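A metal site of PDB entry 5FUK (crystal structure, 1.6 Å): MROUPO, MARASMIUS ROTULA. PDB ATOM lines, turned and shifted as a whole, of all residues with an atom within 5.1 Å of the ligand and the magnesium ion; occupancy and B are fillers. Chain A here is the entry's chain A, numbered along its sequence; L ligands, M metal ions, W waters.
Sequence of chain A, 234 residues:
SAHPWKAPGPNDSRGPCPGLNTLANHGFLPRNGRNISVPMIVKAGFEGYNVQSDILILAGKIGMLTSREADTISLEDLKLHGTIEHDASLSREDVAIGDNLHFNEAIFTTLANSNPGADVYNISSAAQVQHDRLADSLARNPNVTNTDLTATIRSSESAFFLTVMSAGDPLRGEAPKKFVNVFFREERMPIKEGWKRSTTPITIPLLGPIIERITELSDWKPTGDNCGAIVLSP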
ATOM      1  N   PRO A  16      -9.793  -9.989  24.009  1.00  0.00           N
ATOM      2  CA  PRO A  16     -10.011  -9.541  25.367  1.00  0.00           C
ATOM      3  C   PRO A  16      -8.847  -8.789  26.031  1.00  0.00           C
ATOM      4  O   PRO A  16      -8.927  -8.469  27.222  1.00  0.00           O
ATOM      5  CB  PRO A  16     -10.233 -10.885  26.097  1.00  0.00           C
ATOM      6  CG  PRO A  16      -9.292 -11.858  25.385  1.00  0.00           C
ATOM      7  CD  PRO A  16      -9.422 -11.435  23.938  1.00  0.00           C
ATOM      8  N   CYS A  17      -7.776  -8.564  25.293  1.00  0.00           N
ATOM      9  CA  CYS A  17      -6.520  -7.979  25.823  1.00  0.00           C
ATOM     10  C   CYS A  17      -6.398  -6.529  25.345  1.00  0.00           C
ATOM     11  O   CYS A  17      -6.180  -6.259  24.152  1.00  0.00           O
ATOM     12  CB  CYS A  17      -5.331  -8.765  25.321  1.00  0.00           C
ATOM     13  SG  CYS A  17      -3.765  -8.000  25.794  1.00  0.00           S
ATOM     14  N   PRO A  18      -6.418  -5.599  26.274  1.00  0.00           N
ATOM     15  CA  PRO A  18      -6.200  -4.214  25.921  1.00  0.00           C
ATOM     16  C   PRO A  18      -4.848  -3.960  25.398  1.00  0.00           C
ATOM     17  O   PRO A  18      -4.633  -3.061  24.552  1.00  0.00           O
ATOM     18  CB  PRO A  18      -6.429  -3.448  27.234  1.00  0.00           C
ATOM     19  CG  PRO A  18      -6.187  -4.454  28.310  1.00  0.00           C
ATOM     20  CD  PRO A  18      -6.678  -5.770  27.725  1.00  0.00           C
ATOM     21  N   GLY A  19      -3.842  -4.731  25.837  1.00  0.00           N
ATOM     22  CA  GLY A  19      -2.484  -4.499  25.355  1.00  0.00           C
ATOM     23  C   GLY A  19      -2.337  -4.731  23.871  1.00  0.00           C
ATOM     24  O   GLY A  19      -1.791  -3.886  23.103  1.00  0.00           O
ATOM     25  N   LEU A  20      -2.793  -5.916  23.396  1.00  0.00           N
ATOM     26  CA  LEU A  20      -2.684  -6.236  22.034  1.00  0.00           C
ATOM     27  C   LEU A  20      -3.692  -5.450  21.206  1.00  0.00           C
ATOM     28  O   LEU A  20      -3.370  -5.099  20.064  1.00  0.00           O
ATOM     29  CB  LEU A  20      -2.909  -7.739  21.815  1.00  0.00           C
ATOM     30  CG  LEU A  20      -1.954  -8.653  22.581  1.00  0.00           C
ATOM     31  CD1 LEU A  20      -2.330 -10.124  22.324  1.00  0.00           C
ATOM     32  CD2 LEU A  20      -0.548  -8.431  22.100  1.00  0.00           C
ATOM     33  N   LEU A  23      -2.106  -2.096  20.462  1.00  0.00           N
ATOM     34  CA  LEU A  23      -1.052  -2.208  19.460  1.00  0.00           C
ATOM     35  C   LEU A  23      -1.671  -2.304  18.084  1.00  0.00           C
ATOM     36  O   LEU A  23      -1.152  -1.719  17.161  1.00  0.00           O
ATOM     37  CB  LEU A  23      -0.158  -3.404  19.709  1.00  0.00           C
ATOM     38  CG  LEU A  23       0.705  -3.230  20.978  1.00  0.00           C
ATOM     39  CD1 LEU A  23       1.418  -4.554  21.306  1.00  0.00           C
ATOM     40  CD2 LEU A  23       1.761  -2.131  20.856  1.00  0.00           C
ATOM     41  N   ILE A  41       4.196 -10.221  17.627  1.00  0.00           N
ATOM     42  CA  ILE A  41       3.876  -9.724  19.000  1.00  0.00           C
ATOM     43  C   ILE A  41       5.114  -9.209  19.650  1.00  0.00           C
ATOM     44  O   ILE A  41       5.072  -8.161  20.264  1.00  0.00           O
ATOM     45  CB  ILE A  41       3.140 -10.794  19.839  1.00  0.00           C
ATOM     46  CG1 ILE A  41       1.749 -11.127  19.258  1.00  0.00           C
ATOM     47  CG2 ILE A  41       3.058 -10.388  21.283  1.00  0.00           C
ATOM     48  CD1 ILE A  41       1.044 -12.364  19.865  1.00  0.00           C
ATOM     49  N   GLY A  45       5.305  -5.337  20.722  1.00  0.00           N
ATOM     50  CA  GLY A  45       5.406  -4.982  22.155  1.00  0.00           C
ATOM     51  C   GLY A  45       6.638  -4.185  22.439  1.00  0.00           C
ATOM     52  O   GLY A  45       6.658  -3.312  23.261  1.00  0.00           O
ATOM     53  N   TYR A  49       5.647  -0.402  23.491  1.00  0.00           N
ATOM     54  CA  TYR A  49       5.667  -0.313  24.927  1.00  0.00           C
ATOM     55  C   TYR A  49       7.022  -0.512  25.614  1.00  0.00           C
ATOM     56  O   TYR A  49       7.101  -0.314  26.844  1.00  0.00           O
ATOM     57  CB  TYR A  49       4.739  -1.420  25.501  1.00  0.00           C
ATOM     58  CG  TYR A  49       3.271  -1.444  25.055  1.00  0.00           C
ATOM     59  CD1 TYR A  49       2.501  -0.271  24.944  1.00  0.00           C
ATOM     60  CD2 TYR A  49       2.634  -2.671  24.848  1.00  0.00           C
ATOM     61  CE1 TYR A  49       1.163  -0.316  24.608  1.00  0.00           C
ATOM     62  CE2 TYR A  49       1.309  -2.742  24.500  1.00  0.00           C
ATOM     63  CZ  TYR A  49       0.560  -1.571  24.376  1.00  0.00           C
ATOM     64  OH  TYR A  49      -0.749  -1.574  24.053  1.00  0.00           O
ATOM     65  N   VAL A  51       8.263  -3.434  25.988  1.00  0.00           N
ATOM     66  CA  VAL A  51       8.156  -4.737  26.623  1.00  0.00           C
ATOM     67  C   VAL A  51       9.021  -5.719  25.844  1.00  0.00           C
ATOM     68  O   VAL A  51       9.007  -5.771  24.588  1.00  0.00           O
ATOM     69  CB  VAL A  51       6.683  -5.249  26.624  1.00  0.00           C
ATOM     70  CG1 VAL A  51       6.612  -6.666  27.143  1.00  0.00           C
ATOM     71  CG2 VAL A  51       5.827  -4.366  27.509  1.00  0.00           C
ATOM     72  N   LEU A  56       6.800 -11.780  26.291  1.00  0.00           N
ATOM     73  CA  LEU A  56       5.936 -11.867  25.114  1.00  0.00           C
ATOM     74  C   LEU A  56       6.037 -13.228  24.419  1.00  0.00           C
ATOM     75  O   LEU A  56       5.093 -13.676  23.825  1.00  0.00           O
ATOM     76  CB  LEU A  56       6.294 -10.753  24.138  1.00  0.00           C
ATOM     77  CG  LEU A  56       5.931  -9.357  24.702  1.00  0.00           C
ATOM     78  CD1 LEU A  56       6.420  -8.394  23.722  1.00  0.00           C
ATOM     79  CD2 LEU A  56       4.467  -9.201  25.053  1.00  0.00           C
ATOM     80  N   ALA A  59       3.969 -15.659  26.973  1.00  0.00           N
ATOM     81  CA  ALA A  59       2.536 -15.472  26.851  1.00  0.00           C
ATOM     82  C   ALA A  59       2.048 -15.713  25.430  1.00  0.00           C
ATOM     83  O   ALA A  59       0.995 -16.316  25.228  1.00  0.00           O
ATOM     84  CB  ALA A  59       2.155 -14.044  27.270  1.00  0.00           C
ATOM     85  N   GLY A  60       2.816 -15.273  24.480  1.00  0.00           N
ATOM     86  CA  GLY A  60       2.483 -15.420  23.059  1.00  0.00           C
ATOM     87  C   GLY A  60       2.298 -16.847  22.620  1.00  0.00           C
ATOM     88  O   GLY A  60       1.296 -17.170  21.955  1.00  0.00           O
ATOM     89  N   GLY A  63      -0.897 -18.170  23.917  1.00  0.00           N
ATOM     90  CA  GLY A  63      -1.987 -17.585  23.108  1.00  0.00           C
ATOM     91  C   GLY A  63      -2.155 -18.244  21.746  1.00  0.00           C
ATOM     92  O   GLY A  63      -3.312 -18.408  21.267  1.00  0.00           O
ATOM     93  N   ILE A  73      -2.561 -16.381  15.085  1.00  0.00           N
ATOM     94  CA  ILE A  73      -3.913 -16.185  15.633  1.00  0.00           C
ATOM     95  C   ILE A  73      -4.543 -14.957  14.997  1.00  0.00           C
ATOM     96  O   ILE A  73      -3.861 -14.096  14.435  1.00  0.00           O
ATOM     97  CB  ILE A  73      -3.906 -15.925  17.165  1.00  0.00           C
ATOM     98  CG1 ILE A  73      -3.135 -14.660  17.491  1.00  0.00           C
ATOM     99  CG2 ILE A  73      -3.339 -17.138  17.946  1.00  0.00           C
ATOM    100  CD1 ILE A  73      -3.244 -14.282  18.974  1.00  0.00           C
ATOM    101  N   LEU A  78      -8.176 -15.221  21.167  1.00  0.00           N
ATOM    102  CA  LEU A  78      -7.724 -15.164  22.560  1.00  0.00           C
ATOM    103  C   LEU A  78      -8.843 -15.125  23.581  1.00  0.00           C
ATOM    104  O   LEU A  78      -8.597 -15.339  24.786  1.00  0.00           O
ATOM    105  CB  LEU A  78      -6.839 -13.945  22.748  1.00  0.00           C
ATOM    106  CG  LEU A  78      -5.521 -13.932  22.013  1.00  0.00           C
ATOM    107  CD1 LEU A  78      -4.740 -12.621  22.059  1.00  0.00           C
ATOM    108  CD2 LEU A  78      -4.567 -15.070  22.482  1.00  0.00           C
ATOM    109  N   ILE A  84      -5.848 -18.618  28.266  1.00  0.00           N
ATOM    110  CA  ILE A  84      -5.474 -17.459  29.075  1.00  0.00           C
ATOM    111  C   ILE A  84      -6.693 -16.754  29.681  1.00  0.00           C
ATOM    112  O   ILE A  84      -6.717 -16.427  30.814  1.00  0.00           O
ATOM    113  CB  ILE A  84      -4.614 -16.463  28.296  1.00  0.00           C
ATOM    114  CG1 ILE A  84      -3.336 -17.126  27.858  1.00  0.00           C
ATOM    115  CG2 ILE A  84      -4.277 -15.248  29.148  1.00  0.00           C
ATOM    116  CD1 ILE A  84      -2.542 -16.311  26.897  1.00  0.00           C
ATOM    117  N   GLU A  85      -7.705 -16.564  28.872  1.00  0.00           N
ATOM    118  CA  GLU A  85      -8.883 -15.848  29.322  1.00  0.00           C
ATOM    119  C   GLU A  85      -9.432 -16.491  30.522  1.00  0.00           C
ATOM    120  O   GLU A  85      -9.573 -17.721  30.620  1.00  0.00           O
ATOM    121  CB  GLU A  85      -9.924 -15.766  28.240  1.00  0.00           C
ATOM    122  CG  GLU A  85     -10.973 -14.665  28.478  1.00  0.00           C
ATOM    123  CD  GLU A  85     -12.057 -15.147  29.379  1.00  0.00           C
ATOM    124  OE1 GLU A  85     -12.485 -16.319  29.319  1.00  0.00           O
ATOM    125  OE2 GLU A  85     -12.492 -14.400  30.283  1.00  0.00           O
ATOM    126  N   HIS A  86      -9.830 -15.663  31.473  1.00  0.00           N
ATOM    127  CA  HIS A  86     -10.205 -16.121  32.808  1.00  0.00           C
ATOM    128  C   HIS A  86     -11.323 -15.254  33.400  1.00  0.00           C
ATOM    129  O   HIS A  86     -11.601 -14.106  32.980  1.00  0.00           O
ATOM    130  CB  HIS A  86      -9.022 -16.026  33.779  1.00  0.00           C
ATOM    131  CG  HIS A  86      -8.414 -14.689  33.790  1.00  0.00           C
ATOM    132  ND1 HIS A  86      -8.960 -13.619  34.431  1.00  0.00           N
ATOM    133  CD2 HIS A  86      -7.317 -14.226  33.177  1.00  0.00           C
ATOM    134  CE1 HIS A  86      -8.238 -12.538  34.203  1.00  0.00           C
ATOM    135  NE2 HIS A  86      -7.213 -12.889  33.447  1.00  0.00           N
ATOM    136  N   ASP A  87     -12.002 -15.826  34.391  1.00  0.00           N
ATOM    137  CA  ASP A  87     -12.995 -15.054  35.129  1.00  0.00           C
ATOM    138  C   ASP A  87     -12.321 -13.986  36.026  1.00  0.00           C
ATOM    139  O   ASP A  87     -11.091 -14.002  36.206  1.00  0.00           O
ATOM    140  CB  ASP A  87     -13.761 -15.978  36.043  1.00  0.00           C
ATOM    141  CG  ASP A  87     -14.459 -17.095  35.288  1.00  0.00           C
ATOM    142  OD1 ASP A  87     -14.975 -16.856  34.214  1.00  0.00           O
ATOM    143  OD2 ASP A  87     -14.616 -18.191  35.890  1.00  0.00           O
ATOM    144  N   SER A  89     -11.955 -10.796  35.418  1.00  0.00           N
ATOM    145  CA  SER A  89     -11.237  -9.796  34.617  1.00  0.00           C
ATOM    146  C   SER A  89     -11.573  -8.408  35.179  1.00  0.00           C
ATOM    147  O   SER A  89     -12.588  -8.185  35.907  1.00  0.00           O
ATOM    148  CB  SER A  89     -11.611  -9.864  33.135  1.00  0.00           C
ATOM    149  OG  SER A  89     -11.199 -11.096  32.563  1.00  0.00           O
ATOM    150  N   LEU A  90     -10.661  -7.480  34.865  1.00  0.00           N
ATOM    151  CA  LEU A  90     -10.779  -6.101  35.318  1.00  0.00           C
ATOM    152  C   LEU A  90     -11.795  -5.309  34.462  1.00  0.00           C
ATOM    153  O   LEU A  90     -12.350  -4.299  34.961  1.00  0.00           O
ATOM    154  CB  LEU A  90      -9.455  -5.412  35.120  1.00  0.00           C
ATOM    155  CG  LEU A  90      -8.293  -5.974  35.979  1.00  0.00           C
ATOM    156  CD1 LEU A  90      -6.940  -5.474  35.440  1.00  0.00           C
ATOM    157  CD2 LEU A  90      -8.443  -5.648  37.433  1.00  0.00           C
ATOM    158  N   SER A  91     -12.120  -5.810  33.269  1.00  0.00           N
ATOM    159  CA  SER A  91     -12.929  -4.964  32.380  1.00  0.00           C
ATOM    160  C   SER A  91     -13.869  -5.736  31.480  1.00  0.00           C
ATOM    161  O   SER A  91     -14.531  -5.125  30.633  1.00  0.00           O
ATOM    162  CB  SER A  91     -12.064  -4.060  31.486  1.00  0.00           C
ATOM    163  OG  SER A  91     -11.288  -4.794  30.519  1.00  0.00           O
ATOM    164  N   ARG A  92     -13.872  -7.051  31.659  1.00  0.00           N
ATOM    165  CA  ARG A  92     -14.756  -7.949  30.895  1.00  0.00           C
ATOM    166  C   ARG A  92     -15.567  -8.717  31.926  1.00  0.00           C
ATOM    167  O   ARG A  92     -15.240  -8.978  33.112  1.00  0.00           O
ATOM    168  CB  ARG A  92     -13.977  -8.936  30.020  1.00  0.00           C
ATOM    169  CG  ARG A  92     -13.582  -8.502  28.660  1.00  0.00           C
ATOM    170  CD  ARG A  92     -12.733  -7.212  28.537  1.00  0.00           C
ATOM    171  NE  ARG A  92     -12.320  -6.962  27.197  1.00  0.00           N
ATOM    172  CZ  ARG A  92     -11.619  -5.915  26.774  1.00  0.00           C
ATOM    173  NH1 ARG A  92     -11.220  -4.991  27.673  1.00  0.00           N
ATOM    174  NH2 ARG A  92     -11.352  -5.750  25.496  1.00  0.00           N
ATOM    175  N   GLU A  93     -16.702  -9.223  31.399  1.00  0.00           N
ATOM    176  CA  GLU A  93     -17.518 -10.137  32.214  1.00  0.00           C
ATOM    177  C   GLU A  93     -17.036 -11.586  32.155  1.00  0.00           C
ATOM    178  O   GLU A  93     -16.404 -11.983  31.161  1.00  0.00           O
ATOM    179  CB  GLU A  93     -19.012 -10.087  31.723  1.00  0.00           C
ATOM    180  CG  GLU A  93     -19.599  -8.720  31.810  1.00  0.00           C
ATOM    181  CD  GLU A  93     -21.023  -8.611  31.155  1.00  0.00           C
ATOM    182  OE1 GLU A  93     -21.295  -9.157  30.050  1.00  0.00           O
ATOM    183  OE2 GLU A  93     -21.854  -7.874  31.750  1.00  0.00           O
ATOM    184  N   ASN A 100     -17.252 -12.150  27.627  1.00  0.00           N
ATOM    185  CA  ASN A 100     -15.842 -12.205  28.104  1.00  0.00           C
ATOM    186  C   ASN A 100     -14.880 -11.583  27.113  1.00  0.00           C
ATOM    187  O   ASN A 100     -13.654 -11.665  27.306  1.00  0.00           O
ATOM    188  CB  ASN A 100     -15.437 -13.643  28.378  1.00  0.00           C
ATOM    189  CG  ASN A 100     -15.194 -14.434  27.071  1.00  0.00           C
ATOM    190  OD1 ASN A 100     -15.644 -14.041  25.964  1.00  0.00           O
ATOM    191  ND2 ASN A 100     -14.379 -15.502  27.163  1.00  0.00           N
ATOM    192  N   GLU A 157      -1.390  -9.372  34.657  1.00  0.00           N
ATOM    193  CA  GLU A 157      -2.108  -8.382  33.860  1.00  0.00           C
ATOM    194  C   GLU A 157      -2.157  -7.030  34.591  1.00  0.00           C
ATOM    195  O   GLU A 157      -1.949  -5.980  33.979  1.00  0.00           O
ATOM    196  CB  GLU A 157      -3.494  -8.931  33.499  1.00  0.00           C
ATOM    197  CG  GLU A 157      -3.329 -10.023  32.426  1.00  0.00           C
ATOM    198  CD  GLU A 157      -4.476 -11.019  32.276  1.00  0.00           C
ATOM    199  OE1 GLU A 157      -5.408 -10.951  33.064  1.00  0.00           O
ATOM    200  OE2 GLU A 157      -4.352 -11.961  31.396  1.00  0.00           O
ATOM    201  N   PHE A 160       1.163  -5.513  34.159  1.00  0.00           N
ATOM    202  CA  PHE A 160       1.303  -5.014  32.806  1.00  0.00           C
ATOM    203  C   PHE A 160       0.739  -3.591  32.629  1.00  0.00           C
ATOM    204  O   PHE A 160       1.374  -2.740  31.991  1.00  0.00           O
ATOM    205  CB  PHE A 160       0.619  -5.960  31.797  1.00  0.00           C
ATOM    206  CG  PHE A 160       1.552  -6.789  30.921  1.00  0.00           C
ATOM    207  CD1 PHE A 160       2.832  -6.335  30.546  1.00  0.00           C
ATOM    208  CD2 PHE A 160       1.084  -8.006  30.419  1.00  0.00           C
ATOM    209  CE1 PHE A 160       3.645  -7.105  29.710  1.00  0.00           C
ATOM    210  CE2 PHE A 160       1.872  -8.781  29.567  1.00  0.00           C
ATOM    211  CZ  PHE A 160       3.162  -8.325  29.215  1.00  0.00           C
ATOM    212  N   PHE A 161      -0.455  -3.329  33.143  1.00  0.00           N
ATOM    213  CA  PHE A 161      -1.038  -1.990  32.969  1.00  0.00           C
ATOM    214  C   PHE A 161      -0.284  -0.977  33.790  1.00  0.00           C
ATOM    215  O   PHE A 161      -0.006   0.133  33.321  1.00  0.00           O
ATOM    216  CB  PHE A 161      -2.551  -1.916  33.072  1.00  0.00           C
ATOM    217  CG  PHE A 161      -3.106  -1.814  34.436  1.00  0.00           C
ATOM    218  CD1 PHE A 161      -2.970  -0.652  35.228  1.00  0.00           C
ATOM    219  CD2 PHE A 161      -3.831  -2.874  34.966  1.00  0.00           C
ATOM    220  CE1 PHE A 161      -3.465  -0.609  36.553  1.00  0.00           C
ATOM    221  CE2 PHE A 161      -4.353  -2.807  36.247  1.00  0.00           C
ATOM    222  CZ  PHE A 161      -4.196  -1.648  37.025  1.00  0.00           C
ATOM    223  N   VAL A 164       3.349  -0.553  31.807  1.00  0.00           N
ATOM    224  CA  VAL A 164       3.332  -0.069  30.487  1.00  0.00           C
ATOM    225  C   VAL A 164       2.725   1.352  30.424  1.00  0.00           C
ATOM    226  O   VAL A 164       3.127   2.121  29.550  1.00  0.00           O
ATOM    227  CB  VAL A 164       2.548  -1.045  29.541  1.00  0.00           C
ATOM    228  CG1 VAL A 164       2.250  -0.465  28.241  1.00  0.00           C
ATOM    229  CG2 VAL A 164       3.327  -2.317  29.368  1.00  0.00           C
ATOM    230  N   PHE A 183      -6.426   3.718  28.104  1.00  0.00           N
ATOM    231  CA  PHE A 183      -5.925   2.412  27.612  1.00  0.00           C
ATOM    232  C   PHE A 183      -7.062   1.390  27.659  1.00  0.00           C
ATOM    233  O   PHE A 183      -7.276   0.704  26.673  1.00  0.00           O
ATOM    234  CB  PHE A 183      -4.784   1.998  28.552  1.00  0.00           C
ATOM    235  CG  PHE A 183      -4.157   0.655  28.262  1.00  0.00           C
ATOM    236  CD1 PHE A 183      -3.512   0.428  27.077  1.00  0.00           C
ATOM    237  CD2 PHE A 183      -4.192  -0.349  29.227  1.00  0.00           C
ATOM    238  CE1 PHE A 183      -2.894  -0.801  26.862  1.00  0.00           C
ATOM    239  CE2 PHE A 183      -3.600  -1.584  28.997  1.00  0.00           C
ATOM    240  CZ  PHE A 183      -2.951  -1.781  27.834  1.00  0.00           C
ATOM    241  N   PHE A 184      -7.775   1.246  28.783  1.00  0.00           N
ATOM    242  CA  PHE A 184      -8.874   0.275  28.826  1.00  0.00           C
ATOM    243  C   PHE A 184     -10.086   0.717  27.980  1.00  0.00           C
ATOM    244  O   PHE A 184     -10.622  -0.065  27.219  1.00  0.00           O
ATOM    245  CB  PHE A 184      -9.306   0.014  30.244  1.00  0.00           C
ATOM    246  CG  PHE A 184      -8.455  -0.989  30.981  1.00  0.00           C
ATOM    247  CD1 PHE A 184      -8.779  -2.333  30.932  1.00  0.00           C
ATOM    248  CD2 PHE A 184      -7.436  -0.597  31.771  1.00  0.00           C
ATOM    249  CE1 PHE A 184      -8.022  -3.213  31.699  1.00  0.00           C
ATOM    250  CE2 PHE A 184      -6.658  -1.501  32.514  1.00  0.00           C
ATOM    251  CZ  PHE A 184      -6.978  -2.808  32.463  1.00  0.00           C
HETATM  252  C1  LIG L   1      -5.711  -9.512  29.321  1.00  0.00           C
HETATM  253  C2  LIG L   1      -2.305  -6.169  29.098  1.00  0.00           C
HETATM  254  C3  LIG L   1       0.162  -9.000  26.039  1.00  0.00           C
HETATM  255  C4  LIG L   1      -3.412 -12.215  26.114  1.00  0.00           C
HETATM  256  C5  LIG L   1      -4.953  -8.396  29.605  1.00  0.00           C
HETATM  257  C6  LIG L   1      -5.273  -7.455  30.621  1.00  0.00           C
HETATM  258  C7  LIG L   1      -4.294  -6.476  30.538  1.00  0.00           C
HETATM  259  C8  LIG L   1      -3.405  -6.858  29.541  1.00  0.00           C
HETATM  260  C9  LIG L   1      -4.142  -5.253  31.379  1.00  0.00           C
HETATM  261  C10 LIG L   1      -6.402  -7.477  31.581  1.00  0.00           C
HETATM  262  C11 LIG L   1      -7.778  -7.131  30.973  1.00  0.00           C
HETATM  263  C12 LIG L   1      -8.885  -7.372  32.023  1.00  0.00           C
HETATM  264  O1  LIG L   1     -10.029  -6.894  31.796  1.00  0.00           O
HETATM  265  O2  LIG L   1      -8.723  -8.005  33.070  1.00  0.00           O
HETATM  266  C13 LIG L   1      -1.346  -6.622  28.211  1.00  0.00           C
HETATM  267  C14 LIG L   1      -0.194  -5.857  27.814  1.00  0.00           C
HETATM  268  C15 LIG L   1       0.533  -6.646  26.992  1.00  0.00           C
HETATM  269  C16 LIG L   1      -0.240  -7.911  26.811  1.00  0.00           C
HETATM  270  C17 LIG L   1       0.221  -4.449  28.311  1.00  0.00           C
HETATM  271  C18 LIG L   1       1.795  -6.239  26.341  1.00  0.00           C
HETATM  272  C19 LIG L   1       2.041  -6.529  25.075  1.00  0.00           C
HETATM  273  C20 LIG L   1      -0.537 -10.176  25.878  1.00  0.00           C
HETATM  274  C21 LIG L   1      -0.097 -11.300  25.075  1.00  0.00           C
HETATM  275  C22 LIG L   1      -1.130 -12.175  25.109  1.00  0.00           C
HETATM  276  C23 LIG L   1      -2.191 -11.637  25.893  1.00  0.00           C
HETATM  277  C24 LIG L   1       1.250 -11.389  24.432  1.00  0.00           C
HETATM  278  C25 LIG L   1      -1.275 -13.462  24.402  1.00  0.00           C
HETATM  279  C26 LIG L   1      -0.801 -13.692  23.146  1.00  0.00           C
HETATM  280  C27 LIG L   1      -4.360 -11.686  26.952  1.00  0.00           C
HETATM  281  C28 LIG L   1      -5.622 -12.390  27.231  1.00  0.00           C
HETATM  282  C29 LIG L   1      -6.302 -11.604  28.095  1.00  0.00           C
HETATM  283  C30 LIG L   1      -5.400 -10.491  28.417  1.00  0.00           C
HETATM  284  C31 LIG L   1      -6.116 -13.648  26.587  1.00  0.00           C
HETATM  285  C32 LIG L   1      -7.620 -11.865  28.765  1.00  0.00           C
HETATM  286  C33 LIG L   1      -7.527 -12.354  30.199  1.00  0.00           C
HETATM  287  C34 LIG L   1      -8.812 -11.997  30.935  1.00  0.00           C
HETATM  288  O3  LIG L   1      -9.717 -12.879  31.014  1.00  0.00           O
HETATM  289  O4  LIG L   1      -8.949 -10.861  31.435  1.00  0.00           O
HETATM  290  N1  LIG L   1      -3.798  -8.035  28.914  1.00  0.00           N
HETATM  291  N2  LIG L   1      -1.330  -7.822  27.579  1.00  0.00           N
HETATM  292  N3  LIG L   1      -1.801 -10.416  26.346  1.00  0.00           N
HETATM  293  N4  LIG L   1      -4.280 -10.545  27.686  1.00  0.00           N
HETATM  294 FE1  LIG L   1      -2.836  -9.190  27.606  1.00  0.00          FE
HETATM  295 MG    MG M   1     -11.810 -12.685  31.357  1.00  0.00          MG
HETATM  296  O   HOH W   1     -10.400  -9.362  29.383  1.00  0.00           O
HETATM  297  O   HOH W   2     -12.032 -11.529  29.597  1.00  0.00           O
HETATM  298  O   HOH W   3      -7.111  -9.546  34.678  1.00  0.00           O
HETATM  299  O   HOH W   4     -13.767 -12.388  32.016  1.00  0.00           O
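An oxygen (O3) of the ligand lies close to the backbone NH (N) of His 86 (2.8 Å). An oxygen (O4) of the ligand sits close to a ring nitrogen (NE2) of His 86, 3.3 Å away. FE1 of the ligand is bound by SG of Cys 17, 2.4 Å away. The backbone NH (N) of Leu 90 lies within hydrogen-bond range of an oxygen (O2) of the ligand (2.7 Å). The backbone NH (N) of Ser 91 sits at hydrogen-bond distance from an oxygen (O1) of the ligand (2.8 Å). The side-chain hydroxyl of Ser 91 lies within hydrogen-bond range of an oxygen (O1) of the ligand (2.8 Å).
OE1 of Glu 85 lies within hydrogen-bond range of ND2 of Asn 100, at 3.0 Å. NE2 of His 86 sits at hydrogen-bond distance from OE1 of Glu 157, 2.7 Å away. SG of Cys 17 lies close to N of Gly 19. N of Leu 20 lies close to SG of Cys 17 (3.3 Å). The guanidinium group of Arg 92 sits at hydrogen-bond distance from the side-chain hydroxyl of Ser 91. The backbone carbonyl oxygen of Gly 19 is in hydrogen-bond range of the side-chain hydroxyl of Tyr 49, 2.7 Å away.
Residues that only touch the ligand: Glu 157 (3.4 Å), Leu 78 (3.5 Å), Ile 84 (3.5 Å), Pro 18 (3.6 Å), Phe 160 (3.6 Å), Leu 56 (3.6 Å), Gly 19 (3.6 Å), Leu 20 (3.7 Å), Gly 60 (3.7 Å), Ala 59 (3.7 Å), Ile 41 (3.8 Å), Pro 16 (3.8 Å), Arg 92 (3.8 Å), Phe 184 (3.9 Å), Tyr 49 (3.9 Å) and Val 164 (3.9 Å). Hydrophobic or aromatic side chains that line the ligand: Pro 16, Pro 18, Leu 20, Ile 41, Tyr 49, Leu 56, Ala 59, Leu 78, Ile 84, His 86, Leu 90, Phe 160, Val 164 and Phe 184. Within 4 Å of the ligand: Pro 16, Cys 17, Pro 18, Gly 19, Leu 20, Ile 41, Tyr 49, Leu 56, Ala 59, Gly 60, Leu 78, Ile 84, Glu 85, His 86, Ser 89, Leu 90, Ser 91, Arg 92, Glu 157, Phe 160, Val 164 and Phe 184. The nearest printed residue that does not touch the ligand is Phe 161 (4.1 Å).
The magnesium ion is bound by OG of Ser 89 (2.1 Å), water W4 (2.1 Å), water W2 (2.1 Å), O3 of the ligand (2.1 Å), OE2 of Glu 85 (2.1 Å) and O of His 86 (2.2 Å). The magnesium ion has six donor atoms within binding distance.
Water W3 bridges OE1 of Glu 157 and O2 of the ligand. Water W1 lies within hydrogen-bond range of the backbone carbonyl oxygen (O) of Pro 16 (2.8 Å) and an oxygen (O4) of the ligand (2.9 Å).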
